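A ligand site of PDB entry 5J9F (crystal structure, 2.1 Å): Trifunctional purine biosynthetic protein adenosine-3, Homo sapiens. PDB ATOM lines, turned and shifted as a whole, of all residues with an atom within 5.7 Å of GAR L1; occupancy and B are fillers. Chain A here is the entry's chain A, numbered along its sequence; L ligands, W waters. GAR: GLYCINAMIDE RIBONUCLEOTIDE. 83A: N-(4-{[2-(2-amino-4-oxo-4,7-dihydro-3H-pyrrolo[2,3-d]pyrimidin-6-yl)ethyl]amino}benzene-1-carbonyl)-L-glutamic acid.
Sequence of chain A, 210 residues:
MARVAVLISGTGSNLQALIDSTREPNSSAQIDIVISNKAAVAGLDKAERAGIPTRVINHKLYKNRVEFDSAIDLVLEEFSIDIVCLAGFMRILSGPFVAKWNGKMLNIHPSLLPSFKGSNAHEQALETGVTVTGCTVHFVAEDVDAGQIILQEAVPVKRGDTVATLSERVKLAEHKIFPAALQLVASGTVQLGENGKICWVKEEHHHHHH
Thr 11 touches GAR L1. Gly 88 touches GAR L1 (CA to C10, 3.5 Å). Met 90 touches GAR L1. O of Ile 108 touches O8 of GAR L1, at 3.7 Å. His 109 touches GAR L1. Pro 110 touches GAR L1 (CD to O22, 3.4 Å). O of Gly 118 touches N24 of GAR L1, 3.9 Å away. Hydrophobic or aromatic side chains that line GAR L1: Met 90, Ile 108 and Pro 110. 12 residues have an atom within 4 Å of GAR L1: Thr 11, Gly 12, Ser 13, Asn 14, Gly 88, Met 90, Ile 108, His 109, Pro 110, Gly 118, Lys 171 and Glu 174. The nearest printed residue that does not touch GAR L1 is Gly 10 (4.2 Å).
The side-chain hydroxyl (OG) of Ser 13 is in hydrogen-bond range of a ring nitrogen (NE2) of His 175 (2.8 Å). OE2 of Glu 174 sits at hydrogen-bond distance from ND2 of Asn 14 (2.8 Å). The backbone carbonyl oxygen (O) of Lys 171 lies close to a ring nitrogen (ND1) of His 175 (3.2 Å). OD2 of Asp 145 lies close to ND1 of His 109, at 3.4 Å. The backbone NH of Gly 118 sits at hydrogen-bond distance from the side-chain carboxylate of Asp 145.
Water W1 lies within hydrogen-bond range of an oxygen (O16) of GAR L1 (2.6 Å), the backbone carbonyl oxygen (O) of Ala 87 (2.8 Å), the backbone NH (N) of Leu 15 (3.1 Å) and the backbone NH (N) of Asn 14 (3.5 Å). Water W2 bridges an oxygen (O18) of GAR L1 (2.6 Å) and the backbone NH (N) of Thr 11 (2.9 Å). Water W5 lies within hydrogen-bond range of an oxygen (O18) of GAR L1 (2.7 Å), the backbone carbonyl oxygen (O) of Ala 87 (2.9 Å), the backbone NH (N) of Gly 10 (3.1 Å) and the backbone carbonyl oxygen (O) of Gly 88 (3.4 Å). Water W3 lies within hydrogen-bond range of the side-chain carboxylate (OD1) of Asp 145 (2.5 Å), a ring nitrogen (ND1) of His 109 (2.7 Å), a nitrogen (N24) of GAR L1 (2.8 Å), a nitrogen (N5) of 83A L2 (2.9 Å) and the side-chain amide nitrogen (ND2) of Asn 107 (3.0 Å). Water W4 lies within hydrogen-bond range of O of Ile 108, N19 of GAR L1 and N of Gly 88. Water W7 lies within hydrogen-bond range of the side-chain carboxylate (OE1) of Glu 174 (2.7 Å), a ring nitrogen (NE2) of His 122 (2.8 Å), the backbone carbonyl oxygen (O) of Ser 167 (3.0 Å) and an oxygen (O6) of GAR L1 (3.3 Å).
A nitrogen (N24) of GAR L1 lies close to a nitrogen (N5) of 83A L2 (3.2 Å).
An oxygen (O17) of GAR L1 sits at hydrogen-bond distance from the backbone NH (N) of Ser 13 (2.9 Å). OG of Ser 13 lies within hydrogen-bond range of O17 of GAR L1 (2.6 Å). OE1 of Glu 174 sits at hydrogen-bond distance from O6 of GAR L1 (2.7 Å). An oxygen (O18) of GAR L1 lies within hydrogen-bond range of the backbone NH (N) of Gly 12 (2.8 Å). The backbone NH of Asn 14 lies within hydrogen-bond range of an oxygen (O16) of GAR L1, at 2.9 Å. An oxygen (O16) of GAR L1 is in hydrogen-bond range of the side-chain amide nitrogen (ND2) of Asn 14, at 3.0 Å. An oxygen (O17) of GAR L1 lies within salt-bridge range of the side-chain amino group (NZ) of Lys 171, at 3.1 Å. An oxygen (O1) of 83A L2 sits at hydrogen-bond distance from the backbone NH (N) of Asp 145, 2.9 Å away.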
ATOM      1  N   GLY A  10       8.190 -22.814   3.831  1.00  0.00           N
ATOM      2  CA  GLY A  10       9.334 -23.675   4.032  1.00  0.00           C
ATOM      3  C   GLY A  10      10.711 -23.131   3.685  1.00  0.00           C
ATOM      4  O   GLY A  10      11.121 -22.088   4.184  1.00  0.00           O
ATOM      5  N   THR A  11      11.436 -23.839   2.833  1.00  0.00           N
ATOM      6  CA  THR A  11      12.850 -23.514   2.572  1.00  0.00           C
ATOM      7  C   THR A  11      13.125 -22.067   2.111  1.00  0.00           C
ATOM      8  O   THR A  11      14.054 -21.422   2.583  1.00  0.00           O
ATOM      9  CB  THR A  11      13.435 -24.473   1.514  1.00  0.00           C
ATOM     10  OG1 THR A  11      13.152 -25.824   1.885  1.00  0.00           O
ATOM     11  CG2 THR A  11      14.937 -24.265   1.388  1.00  0.00           C
ATOM     12  N   GLY A  12      12.351 -21.585   1.144  1.00  0.00           N
ATOM     13  CA  GLY A  12      12.519 -20.227   0.694  1.00  0.00           C
ATOM     14  C   GLY A  12      13.548 -19.940  -0.382  1.00  0.00           C
ATOM     15  O   GLY A  12      14.029 -18.783  -0.500  1.00  0.00           O
ATOM     16  N   SER A  13      13.867 -20.943  -1.213  1.00  0.00           N
ATOM     17  CA  SER A  13      14.766 -20.683  -2.345  1.00  0.00           C
ATOM     18  C   SER A  13      14.104 -19.727  -3.361  1.00  0.00           C
ATOM     19  O   SER A  13      14.784 -18.880  -3.955  1.00  0.00           O
ATOM     20  CB  SER A  13      15.210 -21.995  -3.021  1.00  0.00           C
ATOM     21  OG  SER A  13      14.155 -22.551  -3.790  1.00  0.00           O
ATOM     22  N   ASN A  14      12.797 -19.852  -3.577  1.00  0.00           N
ATOM     23  CA  ASN A  14      12.121 -18.879  -4.466  1.00  0.00           C
ATOM     24  C   ASN A  14      12.139 -17.453  -3.867  1.00  0.00           C
ATOM     25  O   ASN A  14      12.384 -16.466  -4.571  1.00  0.00           O
ATOM     26  CB  ASN A  14      10.679 -19.295  -4.752  1.00  0.00           C
ATOM     27  CG  ASN A  14      10.602 -20.254  -5.945  1.00  0.00           C
ATOM     28  OD1 ASN A  14      10.758 -19.838  -7.086  1.00  0.00           O
ATOM     29  ND2 ASN A  14      10.413 -21.533  -5.669  1.00  0.00           N
ATOM     30  N   LEU A  15      11.854 -17.358  -2.581  1.00  0.00           N
ATOM     31  CA  LEU A  15      11.973 -16.078  -1.854  1.00  0.00           C
ATOM     32  C   LEU A  15      13.349 -15.457  -2.081  1.00  0.00           C
ATOM     33  O   LEU A  15      13.466 -14.272  -2.424  1.00  0.00           O
ATOM     34  CB  LEU A  15      11.791 -16.284  -0.350  1.00  0.00           C
ATOM     35  CG  LEU A  15      12.209 -15.074   0.508  1.00  0.00           C
ATOM     36  CD1 LEU A  15      11.333 -13.859   0.222  1.00  0.00           C
ATOM     37  CD2 LEU A  15      12.164 -15.423   2.009  1.00  0.00           C
ATOM     38  N   ALA A  87       5.191 -18.195  -2.575  1.00  0.00           N
ATOM     39  CA  ALA A  87       6.498 -18.768  -2.950  1.00  0.00           C
ATOM     40  C   ALA A  87       6.783 -19.959  -2.029  1.00  0.00           C
ATOM     41  O   ALA A  87       7.407 -19.833  -0.979  1.00  0.00           O
ATOM     42  CB  ALA A  87       7.616 -17.688  -2.886  1.00  0.00           C
ATOM     43  N   GLY A  88       6.242 -21.110  -2.418  1.00  0.00           N
ATOM     44  CA  GLY A  88       6.293 -22.309  -1.605  1.00  0.00           C
ATOM     45  C   GLY A  88       5.239 -22.244  -0.517  1.00  0.00           C
ATOM     46  O   GLY A  88       5.350 -22.953   0.475  1.00  0.00           O
ATOM     47  N   PHE A  89       4.241 -21.375  -0.677  1.00  0.00           N
ATOM     48  CA  PHE A  89       3.152 -21.245   0.292  1.00  0.00           C
ATOM     49  C   PHE A  89       2.176 -22.397   0.061  1.00  0.00           C
ATOM     50  O   PHE A  89       1.648 -22.540  -1.039  1.00  0.00           O
ATOM     51  CB  PHE A  89       2.440 -19.903   0.133  1.00  0.00           C
ATOM     52  CG  PHE A  89       1.411 -19.609   1.194  1.00  0.00           C
ATOM     53  CD1 PHE A  89       1.801 -19.357   2.510  1.00  0.00           C
ATOM     54  CD2 PHE A  89       0.060 -19.589   0.875  1.00  0.00           C
ATOM     55  CE1 PHE A  89       0.838 -19.069   3.481  1.00  0.00           C
ATOM     56  CE2 PHE A  89      -0.898 -19.314   1.835  1.00  0.00           C
ATOM     57  CZ  PHE A  89      -0.503 -19.042   3.131  1.00  0.00           C
ATOM     58  N   MET A  90       1.948 -23.230   1.063  1.00  0.00           N
ATOM     59  CA  MET A  90       1.174 -24.450   0.792  1.00  0.00           C
ATOM     60  C   MET A  90      -0.263 -24.455   1.322  1.00  0.00           C
ATOM     61  O   MET A  90      -0.790 -25.522   1.686  1.00  0.00           O
ATOM     62  CB  MET A  90       1.917 -25.672   1.352  1.00  0.00           C
ATOM     63  CG  MET A  90       3.300 -25.913   0.751  1.00  0.00           C
ATOM     64  SD  MET A  90       3.322 -25.967  -1.088  1.00  0.00           S
ATOM     65  CE  MET A  90       2.490 -27.533  -1.420  1.00  0.00           C
ATOM     66  N   ASN A 107       1.470 -16.843  -8.117  1.00  0.00           N
ATOM     67  CA  ASN A 107       1.866 -18.128  -7.518  1.00  0.00           C
ATOM     68  C   ASN A 107       2.913 -18.806  -8.410  1.00  0.00           C
ATOM     69  O   ASN A 107       2.839 -18.661  -9.638  1.00  0.00           O
ATOM     70  CB  ASN A 107       0.658 -19.048  -7.341  1.00  0.00           C
ATOM     71  CG  ASN A 107       1.040 -20.417  -6.780  1.00  0.00           C
ATOM     72  OD1 ASN A 107       1.594 -20.501  -5.687  1.00  0.00           O
ATOM     73  ND2 ASN A 107       0.681 -21.488  -7.510  1.00  0.00           N
ATOM     74  N   ILE A 108       3.872 -19.515  -7.838  1.00  0.00           N
ATOM     75  CA  ILE A 108       4.776 -20.371  -8.655  1.00  0.00           C
ATOM     76  C   ILE A 108       4.351 -21.850  -8.446  1.00  0.00           C
ATOM     77  O   ILE A 108       4.113 -22.290  -7.302  1.00  0.00           O
ATOM     78  CB  ILE A 108       6.279 -20.126  -8.308  1.00  0.00           C
ATOM     79  CG1 ILE A 108       7.216 -21.024  -9.127  1.00  0.00           C
ATOM     80  CG2 ILE A 108       6.566 -20.389  -6.817  1.00  0.00           C
ATOM     81  CD1 ILE A 108       7.406 -20.625 -10.555  1.00  0.00           C
ATOM     82  N   HIS A 109       4.207 -22.597  -9.534  1.00  0.00           N
ATOM     83  CA  HIS A 109       3.747 -23.996  -9.472  1.00  0.00           C
ATOM     84  C   HIS A 109       4.717 -24.886 -10.313  1.00  0.00           C
ATOM     85  O   HIS A 109       5.034 -24.561 -11.469  1.00  0.00           O
ATOM     86  CB  HIS A 109       2.313 -24.124  -9.998  1.00  0.00           C
ATOM     87  CG  HIS A 109       1.787 -25.538  -9.970  1.00  0.00           C
ATOM     88  ND1 HIS A 109       1.213 -26.098  -8.853  1.00  0.00           N
ATOM     89  CD2 HIS A 109       1.799 -26.505 -10.917  1.00  0.00           C
ATOM     90  CE1 HIS A 109       0.859 -27.344  -9.109  1.00  0.00           C
ATOM     91  NE2 HIS A 109       1.232 -27.625 -10.352  1.00  0.00           N
ATOM     92  N   PRO A 110       5.195 -26.003  -9.724  1.00  0.00           N
ATOM     93  CA  PRO A 110       6.280 -26.768 -10.373  1.00  0.00           C
ATOM     94  C   PRO A 110       5.759 -27.791 -11.370  1.00  0.00           C
ATOM     95  O   PRO A 110       6.159 -28.972 -11.314  1.00  0.00           O
ATOM     96  CB  PRO A 110       6.971 -27.475  -9.185  1.00  0.00           C
ATOM     97  CG  PRO A 110       5.879 -27.655  -8.153  1.00  0.00           C
ATOM     98  CD  PRO A 110       4.916 -26.457  -8.359  1.00  0.00           C
ATOM     99  N   GLY A 118      -2.109 -29.140  -8.233  1.00  0.00           N
ATOM    100  CA  GLY A 118      -2.123 -29.639  -6.876  1.00  0.00           C
ATOM    101  C   GLY A 118      -0.754 -29.686  -6.228  1.00  0.00           C
ATOM    102  O   GLY A 118       0.212 -29.164  -6.781  1.00  0.00           O
ATOM    103  N   SER A 119      -0.668 -30.365  -5.078  1.00  0.00           N
ATOM    104  CA  SER A 119       0.443 -30.140  -4.165  1.00  0.00           C
ATOM    105  C   SER A 119       1.609 -31.112  -4.330  1.00  0.00           C
ATOM    106  O   SER A 119       2.642 -30.923  -3.674  1.00  0.00           O
ATOM    107  CB  SER A 119      -0.046 -30.228  -2.725  1.00  0.00           C
ATOM    108  OG  SER A 119      -0.483 -31.545  -2.477  1.00  0.00           O
ATOM    109  N   HIS A 122       5.434 -33.018  -8.863  1.00  0.00           N
ATOM    110  CA  HIS A 122       6.529 -33.891  -9.340  1.00  0.00           C
ATOM    111  C   HIS A 122       6.170 -35.365  -9.262  1.00  0.00           C
ATOM    112  O   HIS A 122       6.552 -36.140 -10.140  1.00  0.00           O
ATOM    113  CB  HIS A 122       7.801 -33.625  -8.534  1.00  0.00           C
ATOM    114  CG  HIS A 122       8.327 -32.232  -8.687  1.00  0.00           C
ATOM    115  ND1 HIS A 122       8.647 -31.690  -9.919  1.00  0.00           N
ATOM    116  CD2 HIS A 122       8.559 -31.265  -7.760  1.00  0.00           C
ATOM    117  CE1 HIS A 122       9.067 -30.447  -9.740  1.00  0.00           C
ATOM    118  NE2 HIS A 122       9.023 -30.156  -8.451  1.00  0.00           N
ATOM    119  N   ASP A 145      -4.722 -23.350  -8.986  1.00  0.00           N
ATOM    120  CA  ASP A 145      -3.768 -23.583 -10.080  1.00  0.00           C
ATOM    121  C   ASP A 145      -4.436 -23.452 -11.437  1.00  0.00           C
ATOM    122  O   ASP A 145      -4.040 -24.111 -12.410  1.00  0.00           O
ATOM    123  CB  ASP A 145      -3.116 -24.993  -9.987  1.00  0.00           C
ATOM    124  CG  ASP A 145      -2.290 -25.198  -8.701  1.00  0.00           C
ATOM    125  OD1 ASP A 145      -1.821 -24.187  -8.083  1.00  0.00           O
ATOM    126  OD2 ASP A 145      -2.115 -26.375  -8.305  1.00  0.00           O
ATOM    127  N   SER A 167      12.912 -31.989  -8.690  1.00  0.00           N
ATOM    128  CA  SER A 167      12.530 -30.714  -8.126  1.00  0.00           C
ATOM    129  C   SER A 167      13.732 -29.780  -8.073  1.00  0.00           C
ATOM    130  O   SER A 167      13.569 -28.572  -8.207  1.00  0.00           O
ATOM    131  CB  SER A 167      11.929 -30.870  -6.717  1.00  0.00           C
ATOM    132  OG  SER A 167      12.834 -31.557  -5.890  1.00  0.00           O
ATOM    133  N   LYS A 171      13.553 -26.201  -9.866  1.00  0.00           N
ATOM    134  CA  LYS A 171      13.746 -24.961  -9.074  1.00  0.00           C
ATOM    135  C   LYS A 171      14.704 -24.003  -9.752  1.00  0.00           C
ATOM    136  O   LYS A 171      14.565 -22.788  -9.602  1.00  0.00           O
ATOM    137  CB  LYS A 171      14.252 -25.284  -7.661  1.00  0.00           C
ATOM    138  CG  LYS A 171      13.131 -25.738  -6.723  1.00  0.00           C
ATOM    139  CD  LYS A 171      13.597 -25.883  -5.253  1.00  0.00           C
ATOM    140  CE  LYS A 171      12.470 -26.438  -4.348  1.00  0.00           C
ATOM    141  NZ  LYS A 171      12.756 -26.297  -2.855  1.00  0.00           N
ATOM    142  N   GLU A 174      12.418 -22.183 -11.812  1.00  0.00           N
ATOM    143  CA  GLU A 174      11.487 -21.361 -11.039  1.00  0.00           C
ATOM    144  C   GLU A 174      12.163 -20.060 -10.682  1.00  0.00           C
ATOM    145  O   GLU A 174      11.547 -18.987 -10.748  1.00  0.00           O
ATOM    146  CB  GLU A 174      11.038 -22.082  -9.760  1.00  0.00           C
ATOM    147  CG  GLU A 174      10.202 -23.332  -9.997  1.00  0.00           C
ATOM    148  CD  GLU A 174       9.861 -24.041  -8.643  1.00  0.00           C
ATOM    149  OE1 GLU A 174       9.877 -25.289  -8.542  1.00  0.00           O
ATOM    150  OE2 GLU A 174       9.590 -23.315  -7.668  1.00  0.00           O
ATOM    151  N   HIS A 175      13.445 -20.161 -10.302  1.00  0.00           N
ATOM    152  CA  HIS A 175      14.185 -18.997  -9.850  1.00  0.00           C
ATOM    153  C   HIS A 175      14.466 -17.977 -10.955  1.00  0.00           C
ATOM    154  O   HIS A 175      14.908 -16.898 -10.669  1.00  0.00           O
ATOM    155  CB  HIS A 175      15.517 -19.418  -9.234  1.00  0.00           C
ATOM    156  CG  HIS A 175      15.358 -20.253  -8.018  1.00  0.00           C
ATOM    157  ND1 HIS A 175      16.360 -21.082  -7.546  1.00  0.00           N
ATOM    158  CD2 HIS A 175      14.296 -20.429  -7.190  1.00  0.00           C
ATOM    159  CE1 HIS A 175      15.929 -21.714  -6.470  1.00  0.00           C
ATOM    160  NE2 HIS A 175      14.689 -21.337  -6.225  1.00  0.00           N
HETATM  161  C1  GAR L   1       8.772 -24.816  -5.085  1.00  0.00           C
HETATM  162  O6  GAR L   1       9.200 -25.815  -5.993  1.00  0.00           O
HETATM  163  C2  GAR L   1       7.375 -24.431  -5.519  1.00  0.00           C
HETATM  164  O8  GAR L   1       7.207 -24.364  -6.928  1.00  0.00           O
HETATM  165  C3  GAR L   1       6.507 -25.522  -4.900  1.00  0.00           C
HETATM  166  O4  GAR L   1       7.122 -25.668  -3.636  1.00  0.00           O
HETATM  167  C5  GAR L   1       8.538 -25.429  -3.715  1.00  0.00           C
HETATM  168  C10 GAR L   1       8.905 -24.428  -2.631  1.00  0.00           C
HETATM  169  O12 GAR L   1      10.327 -24.263  -2.618  1.00  0.00           O
HETATM  170  N19 GAR L   1       5.155 -25.003  -4.738  1.00  0.00           N
HETATM  171  C21 GAR L   1       4.100 -25.792  -4.909  1.00  0.00           C
HETATM  172  O22 GAR L   1       4.180 -27.015  -5.074  1.00  0.00           O
HETATM  173  C23 GAR L   1       2.760 -25.069  -4.886  1.00  0.00           C
HETATM  174  N24 GAR L   1       1.642 -25.990  -4.983  1.00  0.00           N
HETATM  175  P15 GAR L   1      11.051 -23.011  -1.853  1.00  0.00           P
HETATM  176  O16 GAR L   1      10.734 -21.769  -2.701  1.00  0.00           O
HETATM  177  O17 GAR L   1      12.518 -23.401  -1.889  1.00  0.00           O
HETATM  178  O18 GAR L   1      10.439 -22.942  -0.464  1.00  0.00           O
HETATM  179  C1  83A L   2      -3.775 -21.162  -5.209  1.00  0.00           C
HETATM  180  N1  83A L   2      -5.962 -20.553  -5.824  1.00  0.00           N
HETATM  181  O1  83A L   2      -4.437 -20.911  -7.434  1.00  0.00           O
HETATM  182  C2  83A L   2      -4.709 -20.870  -6.200  1.00  0.00           C
HETATM  183  N2  83A L   2      -5.461 -20.764  -3.564  1.00  0.00           N
HETATM  184  O2  83A L   2      -3.620 -29.324  -1.432  1.00  0.00           O
HETATM  185  C3  83A L   2      -6.342 -20.523  -4.540  1.00  0.00           C
HETATM  186  N3  83A L   2      -7.673 -20.174  -4.204  1.00  0.00           N
HETATM  187  O3  83A L   2      -5.699 -28.088   2.695  1.00  0.00           O
HETATM  188  C4  83A L   2      -4.206 -21.091  -3.857  1.00  0.00           C
HETATM  189  N4  83A L   2      -3.180 -21.394  -3.056  1.00  0.00           N
HETATM  190  O4  83A L   2      -4.645 -26.239   2.039  1.00  0.00           O
HETATM  191  C5  83A L   2      -2.047 -21.674  -3.731  1.00  0.00           C
HETATM  192  N5  83A L   2      -0.894 -24.183  -4.328  1.00  0.00           N
HETATM  193  O5  83A L   2      -1.820 -31.309   3.926  1.00  0.00           O
HETATM  194  C6  83A L   2      -2.436 -21.529  -5.073  1.00  0.00           C
HETATM  195  N6  83A L   2      -3.205 -27.752   0.284  1.00  0.00           N
HETATM  196  O6  83A L   2      -0.072 -29.986   3.910  1.00  0.00           O
HETATM  197  C7  83A L   2      -0.732 -22.046  -3.070  1.00  0.00           C
HETATM  198  C8  83A L   2       0.013 -23.137  -3.833  1.00  0.00           C
HETATM  199  C9  83A L   2      -1.492 -25.218  -3.560  1.00  0.00           C
HETATM  200  C10 83A L   2      -2.365 -26.142  -4.157  1.00  0.00           C
HETATM  201  C11 83A L   2      -2.939 -27.136  -3.361  1.00  0.00           C
HETATM  202  C12 83A L   2      -2.603 -27.191  -2.014  1.00  0.00           C
HETATM  203  C13 83A L   2      -1.722 -26.273  -1.452  1.00  0.00           C
HETATM  204  C14 83A L   2      -1.151 -25.285  -2.224  1.00  0.00           C
HETATM  205  C15 83A L   2      -3.190 -28.239  -1.059  1.00  0.00           C
HETATM  206  C16 83A L   2      -3.669 -28.380   1.467  1.00  0.00           C
HETATM  207  C17 83A L   2      -4.733 -27.522   2.094  1.00  0.00           C
HETATM  208  C18 83A L   2      -2.508 -28.499   2.445  1.00  0.00           C
HETATM  209  C19 83A L   2      -1.656 -29.722   2.106  1.00  0.00           C
HETATM  210  C20 83A L   2      -1.151 -30.372   3.389  1.00  0.00           C
HETATM  211  O   HOH W   1      10.193 -19.616  -1.284  1.00  0.00           O
HETATM  212  O   HOH W   2       9.942 -25.246   0.728  1.00  0.00           O
HETATM  213  O   HOH W   3       0.362 -24.447  -6.957  1.00  0.00           O
HETATM  214  O   HOH W   4       4.649 -22.170  -4.744  1.00  0.00           O
HETATM  215  O   HOH W   5       8.513 -21.726   0.894  1.00  0.00           O
HETATM  216  O   HOH W   6       2.989 -29.253  -6.493  1.00  0.00           O
HETATM  217  O   HOH W   7      10.617 -27.871  -8.189  1.00  0.00           O
